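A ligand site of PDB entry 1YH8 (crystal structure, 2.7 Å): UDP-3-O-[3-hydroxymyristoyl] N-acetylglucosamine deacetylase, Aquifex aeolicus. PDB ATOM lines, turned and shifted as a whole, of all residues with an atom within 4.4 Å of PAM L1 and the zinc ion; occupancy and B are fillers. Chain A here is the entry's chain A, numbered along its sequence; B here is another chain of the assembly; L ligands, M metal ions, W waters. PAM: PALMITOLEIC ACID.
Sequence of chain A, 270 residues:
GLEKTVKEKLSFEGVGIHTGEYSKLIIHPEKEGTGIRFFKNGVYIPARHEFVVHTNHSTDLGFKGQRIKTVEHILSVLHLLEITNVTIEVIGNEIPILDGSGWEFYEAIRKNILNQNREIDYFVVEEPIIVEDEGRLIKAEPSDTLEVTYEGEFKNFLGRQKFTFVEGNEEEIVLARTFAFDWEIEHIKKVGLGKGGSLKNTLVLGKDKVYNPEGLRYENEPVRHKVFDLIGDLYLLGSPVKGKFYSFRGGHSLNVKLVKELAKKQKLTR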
ATOM      1  N   ILE A  17     -28.853 -22.228 -30.383  1.00  0.00           N
ATOM      2  CA  ILE A  17     -28.976 -22.356 -28.947  1.00  0.00           C
ATOM      3  C   ILE A  17     -30.383 -22.036 -28.438  1.00  0.00           C
ATOM      4  O   ILE A  17     -30.832 -22.639 -27.467  1.00  0.00           O
ATOM      5  CB  ILE A  17     -27.939 -21.456 -28.224  1.00  0.00           C
ATOM      6  CG1 ILE A  17     -27.876 -21.855 -26.749  1.00  0.00           C
ATOM      7  CG2 ILE A  17     -28.316 -19.986 -28.377  1.00  0.00           C
ATOM      8  CD1 ILE A  17     -26.922 -21.020 -25.929  1.00  0.00           C
ATOM      9  N   HIS A  18     -31.068 -21.109 -29.094  1.00  0.00           N
ATOM     10  CA  HIS A  18     -32.418 -20.742 -28.660  1.00  0.00           C
ATOM     11  C   HIS A  18     -33.556 -21.487 -29.347  1.00  0.00           C
ATOM     12  O   HIS A  18     -34.469 -21.974 -28.679  1.00  0.00           O
ATOM     13  CB  HIS A  18     -32.640 -19.237 -28.842  1.00  0.00           C
ATOM     14  CG  HIS A  18     -31.892 -18.400 -27.845  1.00  0.00           C
ATOM     15  ND1 HIS A  18     -32.039 -18.560 -26.480  1.00  0.00           N
ATOM     16  CD2 HIS A  18     -31.010 -17.383 -28.007  1.00  0.00           C
ATOM     17  CE1 HIS A  18     -31.282 -17.684 -25.857  1.00  0.00           C
ATOM     18  NE2 HIS A  18     -30.642 -16.959 -26.757  1.00  0.00           N
ATOM     19  N   HIS A  57     -31.214 -12.116 -24.069  1.00  0.00           N
ATOM     20  CA  HIS A  57     -30.597 -13.433 -24.230  1.00  0.00           C
ATOM     21  C   HIS A  57     -29.929 -13.644 -25.586  1.00  0.00           C
ATOM     22  O   HIS A  57     -29.373 -14.720 -25.845  1.00  0.00           O
ATOM     23  CB  HIS A  57     -31.641 -14.519 -23.966  1.00  0.00           C
ATOM     24  CG  HIS A  57     -32.419 -14.287 -22.705  1.00  0.00           C
ATOM     25  ND1 HIS A  57     -31.824 -14.303 -21.461  1.00  0.00           N
ATOM     26  CD2 HIS A  57     -33.708 -13.941 -22.509  1.00  0.00           C
ATOM     27  CE1 HIS A  57     -32.720 -13.969 -20.548  1.00  0.00           C
ATOM     28  NE2 HIS A  57     -33.874 -13.741 -21.162  1.00  0.00           N
ATOM     29  N   GLU A  72     -24.492 -12.040 -32.656  1.00  0.00           N
ATOM     30  CA  GLU A  72     -23.335 -11.536 -31.902  1.00  0.00           C
ATOM     31  C   GLU A  72     -22.008 -12.280 -32.022  1.00  0.00           C
ATOM     32  O   GLU A  72     -20.956 -11.650 -32.112  1.00  0.00           O
ATOM     33  CB  GLU A  72     -23.682 -11.415 -30.423  1.00  0.00           C
ATOM     34  CG  GLU A  72     -24.135 -12.730 -29.771  1.00  0.00           C
ATOM     35  CD  GLU A  72     -25.650 -12.848 -29.687  1.00  0.00           C
ATOM     36  OE1 GLU A  72     -26.346 -12.421 -30.642  1.00  0.00           O
ATOM     37  OE2 GLU A  72     -26.139 -13.366 -28.666  1.00  0.00           O
ATOM     38  N   HIS A  73     -22.029 -13.603 -32.017  1.00  0.00           N
ATOM     39  CA  HIS A  73     -20.790 -14.361 -32.088  1.00  0.00           C
ATOM     40  C   HIS A  73     -20.107 -14.334 -33.449  1.00  0.00           C
ATOM     41  O   HIS A  73     -18.889 -14.181 -33.527  1.00  0.00           O
ATOM     42  CB  HIS A  73     -21.031 -15.806 -31.636  1.00  0.00           C
ATOM     43  CG  HIS A  73     -21.435 -15.925 -30.193  1.00  0.00           C
ATOM     44  ND1 HIS A  73     -21.790 -17.123 -29.617  1.00  0.00           N
ATOM     45  CD2 HIS A  73     -21.582 -14.992 -29.228  1.00  0.00           C
ATOM     46  CE1 HIS A  73     -22.132 -16.926 -28.364  1.00  0.00           C
ATOM     47  NE2 HIS A  73     -22.014 -15.640 -28.100  1.00  0.00           N
ATOM     48  N   THR A 178     -20.192 -19.510 -24.104  1.00  0.00           N
ATOM     49  CA  THR A 178     -21.436 -18.930 -23.594  1.00  0.00           C
ATOM     50  C   THR A 178     -21.709 -19.517 -22.213  1.00  0.00           C
ATOM     51  O   THR A 178     -21.453 -20.705 -21.960  1.00  0.00           O
ATOM     52  CB  THR A 178     -22.608 -19.290 -24.503  1.00  0.00           C
ATOM     53  OG1 THR A 178     -22.408 -18.685 -25.778  1.00  0.00           O
ATOM     54  CG2 THR A 178     -23.907 -18.824 -23.906  1.00  0.00           C
ATOM     55  N   ILE A 185     -31.987 -20.617 -16.036  1.00  0.00           N
ATOM     56  CA  ILE A 185     -32.466 -21.584 -16.995  1.00  0.00           C
ATOM     57  C   ILE A 185     -33.964 -21.800 -17.049  1.00  0.00           C
ATOM     58  O   ILE A 185     -34.534 -21.988 -18.119  1.00  0.00           O
ATOM     59  CB  ILE A 185     -31.787 -22.943 -16.797  1.00  0.00           C
ATOM     60  CG1 ILE A 185     -30.271 -22.797 -16.985  1.00  0.00           C
ATOM     61  CG2 ILE A 185     -32.312 -23.946 -17.810  1.00  0.00           C
ATOM     62  CD1 ILE A 185     -29.516 -24.099 -16.862  1.00  0.00           C
ATOM     63  N   ILE A 188     -35.438 -18.832 -19.145  1.00  0.00           N
ATOM     64  CA  ILE A 188     -35.121 -18.968 -20.562  1.00  0.00           C
ATOM     65  C   ILE A 188     -36.061 -19.963 -21.234  1.00  0.00           C
ATOM     66  O   ILE A 188     -36.620 -19.685 -22.283  1.00  0.00           O
ATOM     67  CB  ILE A 188     -33.673 -19.469 -20.782  1.00  0.00           C
ATOM     68  CG1 ILE A 188     -32.688 -18.582 -20.024  1.00  0.00           C
ATOM     69  CG2 ILE A 188     -33.357 -19.493 -22.277  1.00  0.00           C
ATOM     70  CD1 ILE A 188     -32.751 -17.154 -20.413  1.00  0.00           C
ATOM     71  N   GLY A 194     -33.707 -20.823 -25.366  1.00  0.00           N
ATOM     72  CA  GLY A 194     -32.742 -21.816 -24.935  1.00  0.00           C
ATOM     73  C   GLY A 194     -33.063 -23.246 -25.277  1.00  0.00           C
ATOM     74  O   GLY A 194     -32.613 -24.166 -24.591  1.00  0.00           O
ATOM     75  N   GLY A 197     -29.964 -25.331 -25.969  1.00  0.00           N
ATOM     76  CA  GLY A 197     -28.922 -25.301 -24.957  1.00  0.00           C
ATOM     77  C   GLY A 197     -28.582 -26.631 -24.321  1.00  0.00           C
ATOM     78  O   GLY A 197     -29.442 -27.473 -24.089  1.00  0.00           O
ATOM     79  N   SER A 198     -27.291 -26.824 -24.050  1.00  0.00           N
ATOM     80  CA  SER A 198     -26.803 -28.033 -23.406  1.00  0.00           C
ATOM     81  C   SER A 198     -25.427 -27.734 -22.838  1.00  0.00           C
ATOM     82  O   SER A 198     -24.864 -26.672 -23.088  1.00  0.00           O
ATOM     83  CB  SER A 198     -26.701 -29.168 -24.415  1.00  0.00           C
ATOM     84  OG  SER A 198     -25.519 -29.043 -25.189  1.00  0.00           O
ATOM     85  N   THR A 202     -22.948 -24.603 -23.582  1.00  0.00           N
ATOM     86  CA  THR A 202     -23.160 -23.623 -22.539  1.00  0.00           C
ATOM     87  C   THR A 202     -22.485 -24.030 -21.231  1.00  0.00           C
ATOM     88  O   THR A 202     -22.530 -25.204 -20.849  1.00  0.00           O
ATOM     89  CB  THR A 202     -24.666 -23.436 -22.215  1.00  0.00           C
ATOM     90  OG1 THR A 202     -25.403 -23.135 -23.409  1.00  0.00           O
ATOM     91  CG2 THR A 202     -24.857 -22.304 -21.214  1.00  0.00           C
ATOM     92  N   VAL A 204     -22.798 -23.938 -17.582  1.00  0.00           N
ATOM     93  CA  VAL A 204     -23.815 -23.705 -16.581  1.00  0.00           C
ATOM     94  C   VAL A 204     -23.127 -23.548 -15.250  1.00  0.00           C
ATOM     95  O   VAL A 204     -22.440 -24.461 -14.790  1.00  0.00           O
ATOM     96  CB  VAL A 204     -24.802 -24.874 -16.524  1.00  0.00           C
ATOM     97  CG1 VAL A 204     -25.896 -24.567 -15.510  1.00  0.00           C
ATOM     98  CG2 VAL A 204     -25.391 -25.120 -17.902  1.00  0.00           C
ATOM     99  N   HIS A 225     -16.085 -13.864 -22.257  1.00  0.00           N
ATOM    100  CA  HIS A 225     -17.144 -14.053 -23.225  1.00  0.00           C
ATOM    101  C   HIS A 225     -17.961 -12.786 -23.320  1.00  0.00           C
ATOM    102  O   HIS A 225     -18.432 -12.438 -24.403  1.00  0.00           O
ATOM    103  CB  HIS A 225     -18.071 -15.217 -22.835  1.00  0.00           C
ATOM    104  CG  HIS A 225     -19.103 -15.507 -23.872  1.00  0.00           C
ATOM    105  ND1 HIS A 225     -18.807 -16.220 -25.020  1.00  0.00           N
ATOM    106  CD2 HIS A 225     -20.384 -15.081 -24.008  1.00  0.00           C
ATOM    107  CE1 HIS A 225     -19.860 -16.212 -25.822  1.00  0.00           C
ATOM    108  NE2 HIS A 225     -20.831 -15.533 -25.226  1.00  0.00           N
ATOM    109  N   ASP A 229     -18.965 -10.827 -26.680  1.00  0.00           N
ATOM    110  CA  ASP A 229     -20.292 -10.358 -27.054  1.00  0.00           C
ATOM    111  C   ASP A 229     -20.293  -8.863 -27.396  1.00  0.00           C
ATOM    112  O   ASP A 229     -20.751  -8.456 -28.472  1.00  0.00           O
ATOM    113  CB  ASP A 229     -21.302 -10.617 -25.933  1.00  0.00           C
ATOM    114  CG  ASP A 229     -21.744 -12.077 -25.854  1.00  0.00           C
ATOM    115  OD1 ASP A 229     -21.784 -12.756 -26.897  1.00  0.00           O
ATOM    116  OD2 ASP A 229     -22.101 -12.531 -24.737  1.00  0.00           O
ATOM    117  N   HIS A 252     -26.488  -7.354 -23.919  1.00  0.00           N
ATOM    118  CA  HIS A 252     -26.911  -6.984 -25.265  1.00  0.00           C
ATOM    119  C   HIS A 252     -27.752  -5.715 -25.355  1.00  0.00           C
ATOM    120  O   HIS A 252     -27.527  -4.889 -26.232  1.00  0.00           O
ATOM    121  CB  HIS A 252     -27.635  -8.159 -25.917  1.00  0.00           C
ATOM    122  CG  HIS A 252     -26.764  -9.351 -26.111  1.00  0.00           C
ATOM    123  ND1 HIS A 252     -25.564  -9.288 -26.797  1.00  0.00           N
ATOM    124  CD2 HIS A 252     -26.882 -10.626 -25.672  1.00  0.00           C
ATOM    125  CE1 HIS A 252     -24.985 -10.472 -26.771  1.00  0.00           C
ATOM    126  NE2 HIS A 252     -25.759 -11.306 -26.094  1.00  0.00           N
ATOM    127  N   ILE B 185     -26.131 -33.415 -10.674  1.00  0.00           N
ATOM    128  CA  ILE B 185     -25.618 -33.455 -12.032  1.00  0.00           C
ATOM    129  C   ILE B 185     -24.118 -33.324 -12.177  1.00  0.00           C
ATOM    130  O   ILE B 185     -23.524 -33.982 -13.038  1.00  0.00           O
ATOM    131  CB  ILE B 185     -26.301 -32.389 -12.903  1.00  0.00           C
ATOM    132  CG1 ILE B 185     -27.804 -32.674 -12.968  1.00  0.00           C
ATOM    133  CG2 ILE B 185     -25.740 -32.448 -14.308  1.00  0.00           C
ATOM    134  CD1 ILE B 185     -28.567 -31.689 -13.843  1.00  0.00           C
ATOM    135  N   VAL B 204     -35.261 -32.440 -14.349  1.00  0.00           N
ATOM    136  CA  VAL B 204     -34.273 -31.854 -13.477  1.00  0.00           C
ATOM    137  C   VAL B 204     -35.001 -30.996 -12.462  1.00  0.00           C
ATOM    138  O   VAL B 204     -35.725 -30.070 -12.817  1.00  0.00           O
ATOM    139  CB  VAL B 204     -33.277 -30.995 -14.261  1.00  0.00           C
ATOM    140  CG1 VAL B 204     -32.224 -30.428 -13.315  1.00  0.00           C
ATOM    141  CG2 VAL B 204     -32.624 -31.835 -15.363  1.00  0.00           C
ATOM    142  N   TYR B 211     -36.872 -27.377 -13.650  1.00  0.00           N
ATOM    143  CA  TYR B 211     -36.235 -26.801 -14.837  1.00  0.00           C
ATOM    144  C   TYR B 211     -37.019 -27.076 -16.122  1.00  0.00           C
ATOM    145  O   TYR B 211     -37.205 -26.181 -16.943  1.00  0.00           O
ATOM    146  CB  TYR B 211     -34.806 -27.335 -14.997  1.00  0.00           C
ATOM    147  CG  TYR B 211     -33.811 -26.795 -13.981  1.00  0.00           C
ATOM    148  CD1 TYR B 211     -33.794 -27.279 -12.672  1.00  0.00           C
ATOM    149  CD2 TYR B 211     -32.913 -25.788 -14.330  1.00  0.00           C
ATOM    150  CE1 TYR B 211     -32.905 -26.768 -11.735  1.00  0.00           C
ATOM    151  CE2 TYR B 211     -32.012 -25.275 -13.402  1.00  0.00           C
ATOM    152  CZ  TYR B 211     -32.010 -25.772 -12.103  1.00  0.00           C
ATOM    153  OH  TYR B 211     -31.136 -25.255 -11.160  1.00  0.00           O
HETATM  154  C1  PAM L   1     -24.857 -15.229 -25.688  1.00  0.00           C
HETATM  155  O1  PAM L   1     -24.628 -14.081 -26.192  1.00  0.00           O
HETATM  156  O2  PAM L   1     -23.902 -16.033 -25.340  1.00  0.00           O
HETATM  157  C2  PAM L   1     -26.373 -15.638 -25.516  1.00  0.00           C
HETATM  158  C3  PAM L   1     -26.646 -17.040 -24.923  1.00  0.00           C
HETATM  159  C4  PAM L   1     -27.250 -17.091 -23.494  1.00  0.00           C
HETATM  160  C5  PAM L   1     -28.476 -18.020 -23.426  1.00  0.00           C
HETATM  161  C6  PAM L   1     -28.181 -19.476 -22.997  1.00  0.00           C
HETATM  162  C7  PAM L   1     -29.452 -20.323 -22.965  1.00  0.00           C
HETATM  163  C8  PAM L   1     -29.444 -21.340 -21.837  1.00  0.00           C
HETATM  164  C9  PAM L   1     -28.971 -22.745 -22.218  1.00  0.00           C
HETATM  165  C10 PAM L   1     -29.545 -23.814 -21.294  1.00  0.00           C
HETATM  166  C11 PAM L   1     -28.603 -24.971 -21.043  1.00  0.00           C
HETATM  167  C12 PAM L   1     -29.321 -26.126 -20.361  1.00  0.00           C
HETATM  168  C13 PAM L   1     -28.405 -26.920 -19.435  1.00  0.00           C
HETATM  169  C14 PAM L   1     -29.130 -27.590 -18.186  1.00  0.00           C
HETATM  170  C15 PAM L   1     -29.358 -28.311 -16.893  1.00  0.00           C
HETATM  171  C16 PAM L   1     -29.451 -27.936 -15.541  1.00  0.00           C
HETATM  172  C1  PAM L   2     -33.149 -44.468 -13.459  1.00  0.00           C
HETATM  173  O1  PAM L   2     -33.343 -45.634 -12.985  1.00  0.00           O
HETATM  174  O2  PAM L   2     -34.110 -43.707 -13.871  1.00  0.00           O
HETATM  175  C2  PAM L   2     -31.659 -43.982 -13.533  1.00  0.00           C
HETATM  176  C3  PAM L   2     -31.447 -42.575 -14.120  1.00  0.00           C
HETATM  177  C4  PAM L   2     -30.811 -41.535 -13.189  1.00  0.00           C
HETATM  178  C5  PAM L   2     -29.636 -40.820 -13.856  1.00  0.00           C
HETATM  179  C6  PAM L   2     -30.004 -39.516 -14.545  1.00  0.00           C
HETATM  180  C7  PAM L   2     -28.803 -38.872 -15.184  1.00  0.00           C
HETATM  181  C8  PAM L   2     -28.873 -37.360 -15.064  1.00  0.00           C
HETATM  182  C9  PAM L   2     -28.261 -36.598 -16.239  1.00  0.00           C
HETATM  183  C10 PAM L   2     -28.312 -35.090 -16.007  1.00  0.00           C
HETATM  184  C11 PAM L   2     -29.302 -34.372 -16.905  1.00  0.00           C
HETATM  185  C12 PAM L   2     -28.571 -33.364 -17.774  1.00  0.00           C
HETATM  186  C13 PAM L   2     -29.496 -32.269 -18.302  1.00  0.00           C
HETATM  187  C14 PAM L   2     -28.774 -31.219 -19.229  1.00  0.00           C
HETATM  188  C15 PAM L   2     -28.017 -30.614 -20.387  1.00  0.00           C
HETATM  189  C16 PAM L   2     -26.988 -31.044 -21.239  1.00  0.00           C
HETATM  190 ZN    ZN M   1     -22.306 -14.692 -26.327  1.00  0.00          ZN
HETATM  191  O   HOH W   1     -28.799 -15.074 -21.610  1.00  0.00           O
HETATM  192  O   HOH W   2     -23.548 -16.176 -22.001  1.00  0.00           O
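A ring nitrogen (NE2) of His 252 lies close to an oxygen (O1) of PAM L1 (3.0 Å). O2 of PAM L1 lies close to OG1 of Thr 178 (3.1 Å).
A ring nitrogen (NE2) of His 252 sits at hydrogen-bond distance from the side-chain carboxylate of Glu 72. The backbone carbonyl oxygen (O) of His 57 sits at hydrogen-bond distance from a ring nitrogen (NE2) of His 18, 2.7 Å away. The backbone carbonyl oxygen (O) of Ile 17 is in hydrogen-bond range of the backbone NH (N) of Gly 197. A ring nitrogen (ND1) of His 18 is in hydrogen-bond range of the backbone NH of Gly 194, at 3.0 Å.
The side-chain carboxylate of Glu 72 sits close to an oxygen (O1) of PAM L1 (3.0 Å). CD1 of Ile 17 touches C6 of PAM L1, at 3.5 Å. His 18 touches PAM L1. O of His 57 touches C2 of PAM L1, at 3.2 Å. Ile 185 of chain A touches PAM L1. Gly 197 touches PAM L1 (C to C11, 3.7 Å). Ser 198 touches PAM L1 (N to C11, 3.8 Å). Thr 202 touches PAM L1 (OG1 to C9, 3.8 Å). CG2 of Val 204 of chain A touches C13 of PAM L1, 3.8 Å away. Hydrophobic or aromatic side chains that line PAM L1: Ile 17, His 18, His 73, Ile 185 of chain A, Val 204 of chain A, His 225 and His 252. The nearest printed residue that does not touch PAM L1 is Ile 188 (4.1 Å).
Three residues have an atom within 4 Å of the zinc ion: His 73, His 225 and Asp 229.
The zinc ion is bound by NE2 of His 225, 2.0 Å away. A ring nitrogen (NE2) of His 73 is bound to the zinc ion (2.0 Å). The side-chain carboxylate (OD1) of Asp 229 is bound to the zinc ion (2.1 Å). The zinc ion is bound by an oxygen (O2) of PAM L1 (2.3 Å). The zinc ion is bound by O1 of PAM L1 (2.4 Å). Slightly farther from the zinc ion lies the side-chain carboxylate (OD2) of Asp 229 (2.7 Å).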
